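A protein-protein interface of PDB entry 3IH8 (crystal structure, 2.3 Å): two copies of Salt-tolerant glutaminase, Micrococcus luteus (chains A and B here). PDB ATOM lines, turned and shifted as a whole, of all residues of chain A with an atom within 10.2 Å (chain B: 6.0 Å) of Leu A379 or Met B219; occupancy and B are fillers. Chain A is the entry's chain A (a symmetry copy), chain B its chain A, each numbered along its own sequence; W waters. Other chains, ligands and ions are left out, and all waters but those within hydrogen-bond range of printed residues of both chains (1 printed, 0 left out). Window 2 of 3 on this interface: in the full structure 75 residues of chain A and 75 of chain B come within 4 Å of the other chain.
The backbone carbonyl oxygen (O) of Pro B46 lies close to the side-chain hydroxyl (OG1) of Thr A383.
The guanidinium group (NE) of Arg B49 is in salt-bridge range of the side-chain carboxylate (OD1) of Asp A345 (3.4 Å).
The backbone carbonyl oxygen (O) of Ser A380 lies within hydrogen-bond range of the backbone NH (N) of Gly A385 (3.4 Å).
The side-chain hydroxyl (OG1) of Thr B47 sits at hydrogen-bond distance from the side-chain hydroxyl (OG1) of Thr B45 (3.1 Å).
OG1 of Thr B45 sits at hydrogen-bond distance from N of Arg B49 (2.9 Å).
A ring nitrogen (ND1) of His B217 lies within hydrogen-bond range of the backbone NH (N) of Met B219, at 2.8 Å.
Thr B47 touches Leu A379.
CD2 of Leu A379 touches O of Met B219, 3.6 Å away.
Thr B220 touches Leu A379 (O to CD2, 3.4 Å).
Leu A379 touches Gly B221.
O of Gly B221 touches CB of Ala A382, 3.9 Å away.
Thr A383 touches Thr B47.
Gly A385 touches Thr B47.
Printed residues of chain B within 4 Å of Leu A379: Thr B47 (3.3 Å), Met B219 (3.6 Å), Thr B220 (3.4 Å) and Gly B221 (3.9 Å).
Printed residues of chain B within 4 Å of Ala A382: Gly B221.
Of the printed residues of chain A, Pro B46 touches Thr A383.
Of the printed residues of chain A, Thr B47 touches Leu A379 (3.3 Å), Thr A383 (3.6 Å) and Gly A385 (3.3 Å).
Gly B48 touches none of the printed residues of chain A.
Printed residues of chain A within 4 Å of Arg B49: Asp A345.
His B217 touches none of the printed residues of chain A.
Of the printed residues of chain A, Gly B221 touches Leu A379 (3.9 Å) and Ala A382 (3.9 Å).
The nearest residue of chain A that does not touch Met B219 is Thr A383 (6.1 Å).
Of the 13 printed residues of chain B, 6 touch a printed residue of chain A.
Printed residues of chain B that touch a printed residue of chain A: Pro B46, Thr B47, Arg B49, Met B219, Thr B220 and Gly B221.
Hydrophobic or aromatic side chains of chain B within 4 Å of the printed part of chain A: Pro B46.
Printed residues of chain A that touch a printed residue of chain B: Asp A345, Leu A379, Ala A382, Thr A383 and Gly A385.
Among the printed residues, 9 pairs touch across the chains.
No position is printed for both chains.
Of the 9 pairs that touch across the chains among the printed residues, none has its exchanged pair printed and touching as well.
Water W1 bridges the guanidinium group of Arg B49 and the side-chain carboxylate of Asp A345.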
ATOM      1  N   ASP A 345      -0.169 -27.116 -11.334  1.00  0.00           N
ATOM      2  CA  ASP A 345       1.030 -26.316 -11.566  1.00  0.00           C
ATOM      3  C   ASP A 345       1.035 -25.824 -13.009  1.00  0.00           C
ATOM      4  O   ASP A 345       1.368 -24.663 -13.282  1.00  0.00           O
ATOM      5  CB  ASP A 345       2.297 -27.146 -11.321  1.00  0.00           C
ATOM      6  CG  ASP A 345       2.644 -27.277  -9.846  1.00  0.00           C
ATOM      7  OD1 ASP A 345       3.672 -27.925  -9.536  1.00  0.00           O
ATOM      8  OD2 ASP A 345       1.896 -26.731  -9.005  1.00  0.00           O
ATOM      9  N   ALA A 377      13.579 -26.987 -17.782  1.00  0.00           N
ATOM     10  CA  ALA A 377      13.937 -28.182 -18.534  1.00  0.00           C
ATOM     11  C   ALA A 377      14.786 -29.153 -17.710  1.00  0.00           C
ATOM     12  O   ALA A 377      14.311 -30.219 -17.310  1.00  0.00           O
ATOM     13  CB  ALA A 377      14.683 -27.789 -19.806  1.00  0.00           C
ATOM     14  N   ALA A 378      16.038 -28.779 -17.459  1.00  0.00           N
ATOM     15  CA  ALA A 378      16.968 -29.616 -16.701  1.00  0.00           C
ATOM     16  C   ALA A 378      16.503 -29.931 -15.281  1.00  0.00           C
ATOM     17  O   ALA A 378      16.705 -31.044 -14.796  1.00  0.00           O
ATOM     18  CB  ALA A 378      18.349 -28.960 -16.661  1.00  0.00           C
ATOM     19  N   LEU A 379      15.895 -28.953 -14.615  1.00  0.00           N
ATOM     20  CA  LEU A 379      15.406 -29.149 -13.253  1.00  0.00           C
ATOM     21  C   LEU A 379      14.334 -30.234 -13.291  1.00  0.00           C
ATOM     22  O   LEU A 379      14.344 -31.162 -12.478  1.00  0.00           O
ATOM     23  CB  LEU A 379      14.819 -27.842 -12.702  1.00  0.00           C
ATOM     24  CG  LEU A 379      14.511 -27.697 -11.200  1.00  0.00           C
ATOM     25  CD1 LEU A 379      13.458 -28.706 -10.769  1.00  0.00           C
ATOM     26  CD2 LEU A 379      15.789 -27.876 -10.399  1.00  0.00           C
ATOM     27  N   SER A 380      13.415 -30.111 -14.244  1.00  0.00           N
ATOM     28  CA  SER A 380      12.340 -31.084 -14.411  1.00  0.00           C
ATOM     29  C   SER A 380      12.886 -32.505 -14.466  1.00  0.00           C
ATOM     30  O   SER A 380      12.680 -33.289 -13.544  1.00  0.00           O
ATOM     31  CB  SER A 380      11.561 -30.797 -15.697  1.00  0.00           C
ATOM     32  OG  SER A 380      10.798 -31.927 -16.094  1.00  0.00           O
ATOM     33  N   ALA A 381      13.582 -32.830 -15.552  1.00  0.00           N
ATOM     34  CA  ALA A 381      14.148 -34.163 -15.733  1.00  0.00           C
ATOM     35  C   ALA A 381      14.934 -34.626 -14.508  1.00  0.00           C
ATOM     36  O   ALA A 381      14.888 -35.800 -14.147  1.00  0.00           O
ATOM     37  CB  ALA A 381      15.043 -34.188 -16.971  1.00  0.00           C
ATOM     38  N   ALA A 382      15.651 -33.700 -13.877  1.00  0.00           N
ATOM     39  CA  ALA A 382      16.454 -34.009 -12.693  1.00  0.00           C
ATOM     40  C   ALA A 382      15.571 -34.568 -11.583  1.00  0.00           C
ATOM     41  O   ALA A 382      16.009 -35.384 -10.774  1.00  0.00           O
ATOM     42  CB  ALA A 382      17.182 -32.751 -12.207  1.00  0.00           C
ATOM     43  N   THR A 383      14.322 -34.121 -11.559  1.00  0.00           N
ATOM     44  CA  THR A 383      13.360 -34.571 -10.565  1.00  0.00           C
ATOM     45  C   THR A 383      12.353 -35.529 -11.202  1.00  0.00           C
ATOM     46  O   THR A 383      12.358 -36.729 -10.926  1.00  0.00           O
ATOM     47  CB  THR A 383      12.592 -33.386  -9.972  1.00  0.00           C
ATOM     48  OG1 THR A 383      13.512 -32.493  -9.325  1.00  0.00           O
ATOM     49  CG2 THR A 383      11.560 -33.882  -8.975  1.00  0.00           C
ATOM     50  N   GLY A 384      11.493 -34.983 -12.055  1.00  0.00           N
ATOM     51  CA  GLY A 384      10.489 -35.784 -12.731  1.00  0.00           C
ATOM     52  C   GLY A 384       9.212 -34.995 -12.935  1.00  0.00           C
ATOM     53  O   GLY A 384       8.115 -35.500 -12.696  1.00  0.00           O
ATOM     54  N   GLY A 385       9.358 -33.751 -13.382  1.00  0.00           N
ATOM     55  CA  GLY A 385       8.205 -32.896 -13.599  1.00  0.00           C
ATOM     56  C   GLY A 385       7.514 -33.092 -14.934  1.00  0.00           C
ATOM     57  O   GLY A 385       6.554 -32.388 -15.249  1.00  0.00           O
ATOM     58  N   GLY A 386       8.001 -34.045 -15.724  1.00  0.00           N
ATOM     59  CA  GLY A 386       7.399 -34.309 -17.018  1.00  0.00           C
ATOM     60  C   GLY A 386       7.312 -33.089 -17.920  1.00  0.00           C
ATOM     61  O   GLY A 386       8.310 -32.403 -18.151  1.00  0.00           O
ATOM     62  N   ALA A 387       6.113 -32.818 -18.428  1.00  0.00           N
ATOM     63  CA  ALA A 387       5.897 -31.682 -19.320  1.00  0.00           C
ATOM     64  C   ALA A 387       5.252 -30.492 -18.617  1.00  0.00           C
ATOM     65  O   ALA A 387       4.593 -29.669 -19.258  1.00  0.00           O
ATOM     66  CB  ALA A 387       5.043 -32.111 -20.514  1.00  0.00           C
ATOM     67  N   VAL A 388       5.443 -30.402 -17.303  1.00  0.00           N
ATOM     68  CA  VAL A 388       4.886 -29.300 -16.524  1.00  0.00           C
ATOM     69  C   VAL A 388       5.614 -28.006 -16.889  1.00  0.00           C
ATOM     70  O   VAL A 388       5.020 -26.927 -16.915  1.00  0.00           O
ATOM     71  CB  VAL A 388       5.020 -29.565 -15.000  1.00  0.00           C
ATOM     72  CG1 VAL A 388       4.538 -28.353 -14.209  1.00  0.00           C
ATOM     73  CG2 VAL A 388       4.202 -30.794 -14.612  1.00  0.00           C
ATOM     74  N   HIS A 389       6.902 -28.137 -17.185  1.00  0.00           N
ATOM     75  CA  HIS A 389       7.737 -27.003 -17.558  1.00  0.00           C
ATOM     76  C   HIS A 389       7.283 -26.345 -18.866  1.00  0.00           C
ATOM     77  O   HIS A 389       7.554 -25.167 -19.107  1.00  0.00           O
ATOM     78  CB  HIS A 389       9.200 -27.452 -17.681  1.00  0.00           C
ATOM     79  CG  HIS A 389       9.420 -28.560 -18.669  1.00  0.00           C
ATOM     80  ND1 HIS A 389      10.663 -29.106 -18.905  1.00  0.00           N
ATOM     81  CD2 HIS A 389       8.561 -29.216 -19.485  1.00  0.00           C
ATOM     82  CE1 HIS A 389      10.560 -30.049 -19.823  1.00  0.00           C
ATOM     83  NE2 HIS A 389       9.295 -30.137 -20.192  1.00  0.00           N
ATOM     84  N   ALA B  44       6.107 -29.302   0.411  1.00  0.00           N
ATOM     85  CA  ALA B  44       7.051 -29.151  -0.699  1.00  0.00           C
ATOM     86  C   ALA B  44       6.947 -30.339  -1.632  1.00  0.00           C
ATOM     87  O   ALA B  44       7.031 -31.472  -1.193  1.00  0.00           O
ATOM     88  CB  ALA B  44       8.481 -29.016  -0.181  1.00  0.00           C
ATOM     89  N   THR B  45       6.776 -30.069  -2.925  1.00  0.00           N
ATOM     90  CA  THR B  45       6.648 -31.124  -3.937  1.00  0.00           C
ATOM     91  C   THR B  45       8.005 -31.525  -4.516  1.00  0.00           C
ATOM     92  O   THR B  45       8.996 -30.829  -4.313  1.00  0.00           O
ATOM     93  CB  THR B  45       5.749 -30.650  -5.098  1.00  0.00           C
ATOM     94  OG1 THR B  45       6.408 -29.587  -5.801  1.00  0.00           O
ATOM     95  CG2 THR B  45       4.407 -30.148  -4.563  1.00  0.00           C
ATOM     96  N   PRO B  46       8.062 -32.653  -5.252  1.00  0.00           N
ATOM     97  CA  PRO B  46       9.301 -33.155  -5.869  1.00  0.00           C
ATOM     98  C   PRO B  46       9.870 -32.164  -6.888  1.00  0.00           C
ATOM     99  O   PRO B  46      11.075 -31.887  -6.909  1.00  0.00           O
ATOM    100  CB  PRO B  46       8.853 -34.446  -6.550  1.00  0.00           C
ATOM    101  CG  PRO B  46       7.666 -34.879  -5.734  1.00  0.00           C
ATOM    102  CD  PRO B  46       6.947 -33.588  -5.491  1.00  0.00           C
ATOM    103  N   THR B  47       8.986 -31.639  -7.731  1.00  0.00           N
ATOM    104  CA  THR B  47       9.365 -30.686  -8.761  1.00  0.00           C
ATOM    105  C   THR B  47       9.992 -29.403  -8.205  1.00  0.00           C
ATOM    106  O   THR B  47      10.811 -28.769  -8.872  1.00  0.00           O
ATOM    107  CB  THR B  47       8.145 -30.329  -9.611  1.00  0.00           C
ATOM    108  OG1 THR B  47       6.977 -30.308  -8.779  1.00  0.00           O
ATOM    109  CG2 THR B  47       7.953 -31.355 -10.708  1.00  0.00           C
ATOM    110  N   GLY B  48       9.607 -29.023  -6.991  1.00  0.00           N
ATOM    111  CA  GLY B  48      10.177 -27.832  -6.391  1.00  0.00           C
ATOM    112  C   GLY B  48       9.199 -26.759  -5.949  1.00  0.00           C
ATOM    113  O   GLY B  48       9.603 -25.627  -5.678  1.00  0.00           O
ATOM    114  N   ARG B  49       7.917 -27.094  -5.874  1.00  0.00           N
ATOM    115  CA  ARG B  49       6.930 -26.112  -5.446  1.00  0.00           C
ATOM    116  C   ARG B  49       6.837 -26.182  -3.927  1.00  0.00           C
ATOM    117  O   ARG B  49       7.039 -27.246  -3.336  1.00  0.00           O
ATOM    118  CB  ARG B  49       5.559 -26.413  -6.066  1.00  0.00           C
ATOM    119  CG  ARG B  49       5.582 -26.607  -7.577  1.00  0.00           C
ATOM    120  CD  ARG B  49       5.781 -25.312  -8.328  1.00  0.00           C
ATOM    121  NE  ARG B  49       6.113 -25.557  -9.732  1.00  0.00           N
ATOM    122  CZ  ARG B  49       6.004 -24.649 -10.700  1.00  0.00           C
ATOM    123  NH1 ARG B  49       5.568 -23.428 -10.419  1.00  0.00           N
ATOM    124  NH2 ARG B  49       6.333 -24.957 -11.947  1.00  0.00           N
ATOM    125  N   LEU B  50       6.538 -25.048  -3.301  1.00  0.00           N
ATOM    126  CA  LEU B  50       6.412 -24.981  -1.853  1.00  0.00           C
ATOM    127  C   LEU B  50       5.146 -24.233  -1.454  1.00  0.00           C
ATOM    128  O   LEU B  50       5.089 -23.009  -1.528  1.00  0.00           O
ATOM    129  CB  LEU B  50       7.624 -24.279  -1.259  1.00  0.00           C
ATOM    130  CG  LEU B  50       7.690 -24.160   0.261  1.00  0.00           C
ATOM    131  CD1 LEU B  50       7.885 -25.529   0.875  1.00  0.00           C
ATOM    132  CD2 LEU B  50       8.848 -23.240   0.640  1.00  0.00           C
ATOM    133  N   VAL B 206      10.866 -28.932   2.981  1.00  0.00           N
ATOM    134  CA  VAL B 206      11.888 -29.119   1.962  1.00  0.00           C
ATOM    135  C   VAL B 206      12.774 -30.315   2.294  1.00  0.00           C
ATOM    136  O   VAL B 206      13.078 -31.143   1.426  1.00  0.00           O
ATOM    137  CB  VAL B 206      12.758 -27.848   1.786  1.00  0.00           C
ATOM    138  CG1 VAL B 206      13.876 -28.105   0.775  1.00  0.00           C
ATOM    139  CG2 VAL B 206      11.888 -26.698   1.295  1.00  0.00           C
ATOM    140  N   HIS B 217      17.389 -33.101  -4.111  1.00  0.00           N
ATOM    141  CA  HIS B 217      16.856 -31.839  -3.622  1.00  0.00           C
ATOM    142  C   HIS B 217      15.875 -31.312  -4.648  1.00  0.00           C
ATOM    143  O   HIS B 217      16.219 -31.118  -5.809  1.00  0.00           O
ATOM    144  CB  HIS B 217      17.940 -30.792  -3.397  1.00  0.00           C
ATOM    145  CG  HIS B 217      17.464 -29.641  -2.572  1.00  0.00           C
ATOM    146  ND1 HIS B 217      16.474 -28.784  -2.999  1.00  0.00           N
ATOM    147  CD2 HIS B 217      17.768 -29.264  -1.309  1.00  0.00           C
ATOM    148  CE1 HIS B 217      16.188 -27.928  -2.034  1.00  0.00           C
ATOM    149  NE2 HIS B 217      16.960 -28.198  -0.997  1.00  0.00           N
ATOM    150  N   PRO B 218      14.632 -31.061  -4.220  1.00  0.00           N
ATOM    151  CA  PRO B 218      13.567 -30.561  -5.091  1.00  0.00           C
ATOM    152  C   PRO B 218      13.771 -29.175  -5.704  1.00  0.00           C
ATOM    153  O   PRO B 218      13.223 -28.884  -6.766  1.00  0.00           O
ATOM    154  CB  PRO B 218      12.338 -30.627  -4.188  1.00  0.00           C
ATOM    155  CG  PRO B 218      12.914 -30.290  -2.848  1.00  0.00           C
ATOM    156  CD  PRO B 218      14.186 -31.111  -2.816  1.00  0.00           C
ATOM    157  N   MET B 219      14.563 -28.327  -5.057  1.00  0.00           N
ATOM    158  CA  MET B 219      14.774 -26.980  -5.574  1.00  0.00           C
ATOM    159  C   MET B 219      15.916 -26.839  -6.564  1.00  0.00           C
ATOM    160  O   MET B 219      15.924 -25.907  -7.365  1.00  0.00           O
ATOM    161  CB  MET B 219      15.003 -25.996  -4.429  1.00  0.00           C
ATOM    162  CG  MET B 219      13.939 -26.034  -3.355  1.00  0.00           C
ATOM    163  SD  MET B 219      12.321 -25.966  -4.069  1.00  0.00           S
ATOM    164  CE  MET B 219      11.301 -26.389  -2.648  1.00  0.00           C
ATOM    165  N   THR B 220      16.880 -27.753  -6.523  1.00  0.00           N
ATOM    166  CA  THR B 220      18.020 -27.653  -7.427  1.00  0.00           C
ATOM    167  C   THR B 220      18.218 -28.897  -8.283  1.00  0.00           C
ATOM    168  O   THR B 220      18.830 -28.836  -9.347  1.00  0.00           O
ATOM    169  CB  THR B 220      19.303 -27.353  -6.637  1.00  0.00           C
ATOM    170  OG1 THR B 220      19.821 -28.564  -6.072  1.00  0.00           O
ATOM    171  CG2 THR B 220      18.994 -26.382  -5.502  1.00  0.00           C
ATOM    172  N   GLY B 221      17.699 -30.026  -7.820  1.00  0.00           N
ATOM    173  CA  GLY B 221      17.830 -31.251  -8.583  1.00  0.00           C
ATOM    174  C   GLY B 221      19.119 -31.998  -8.331  1.00  0.00           C
ATOM    175  O   GLY B 221      19.412 -32.988  -9.004  1.00  0.00           O
HETATM  176  O   HOH W   1       3.090 -24.195 -10.513  1.00  0.00           O
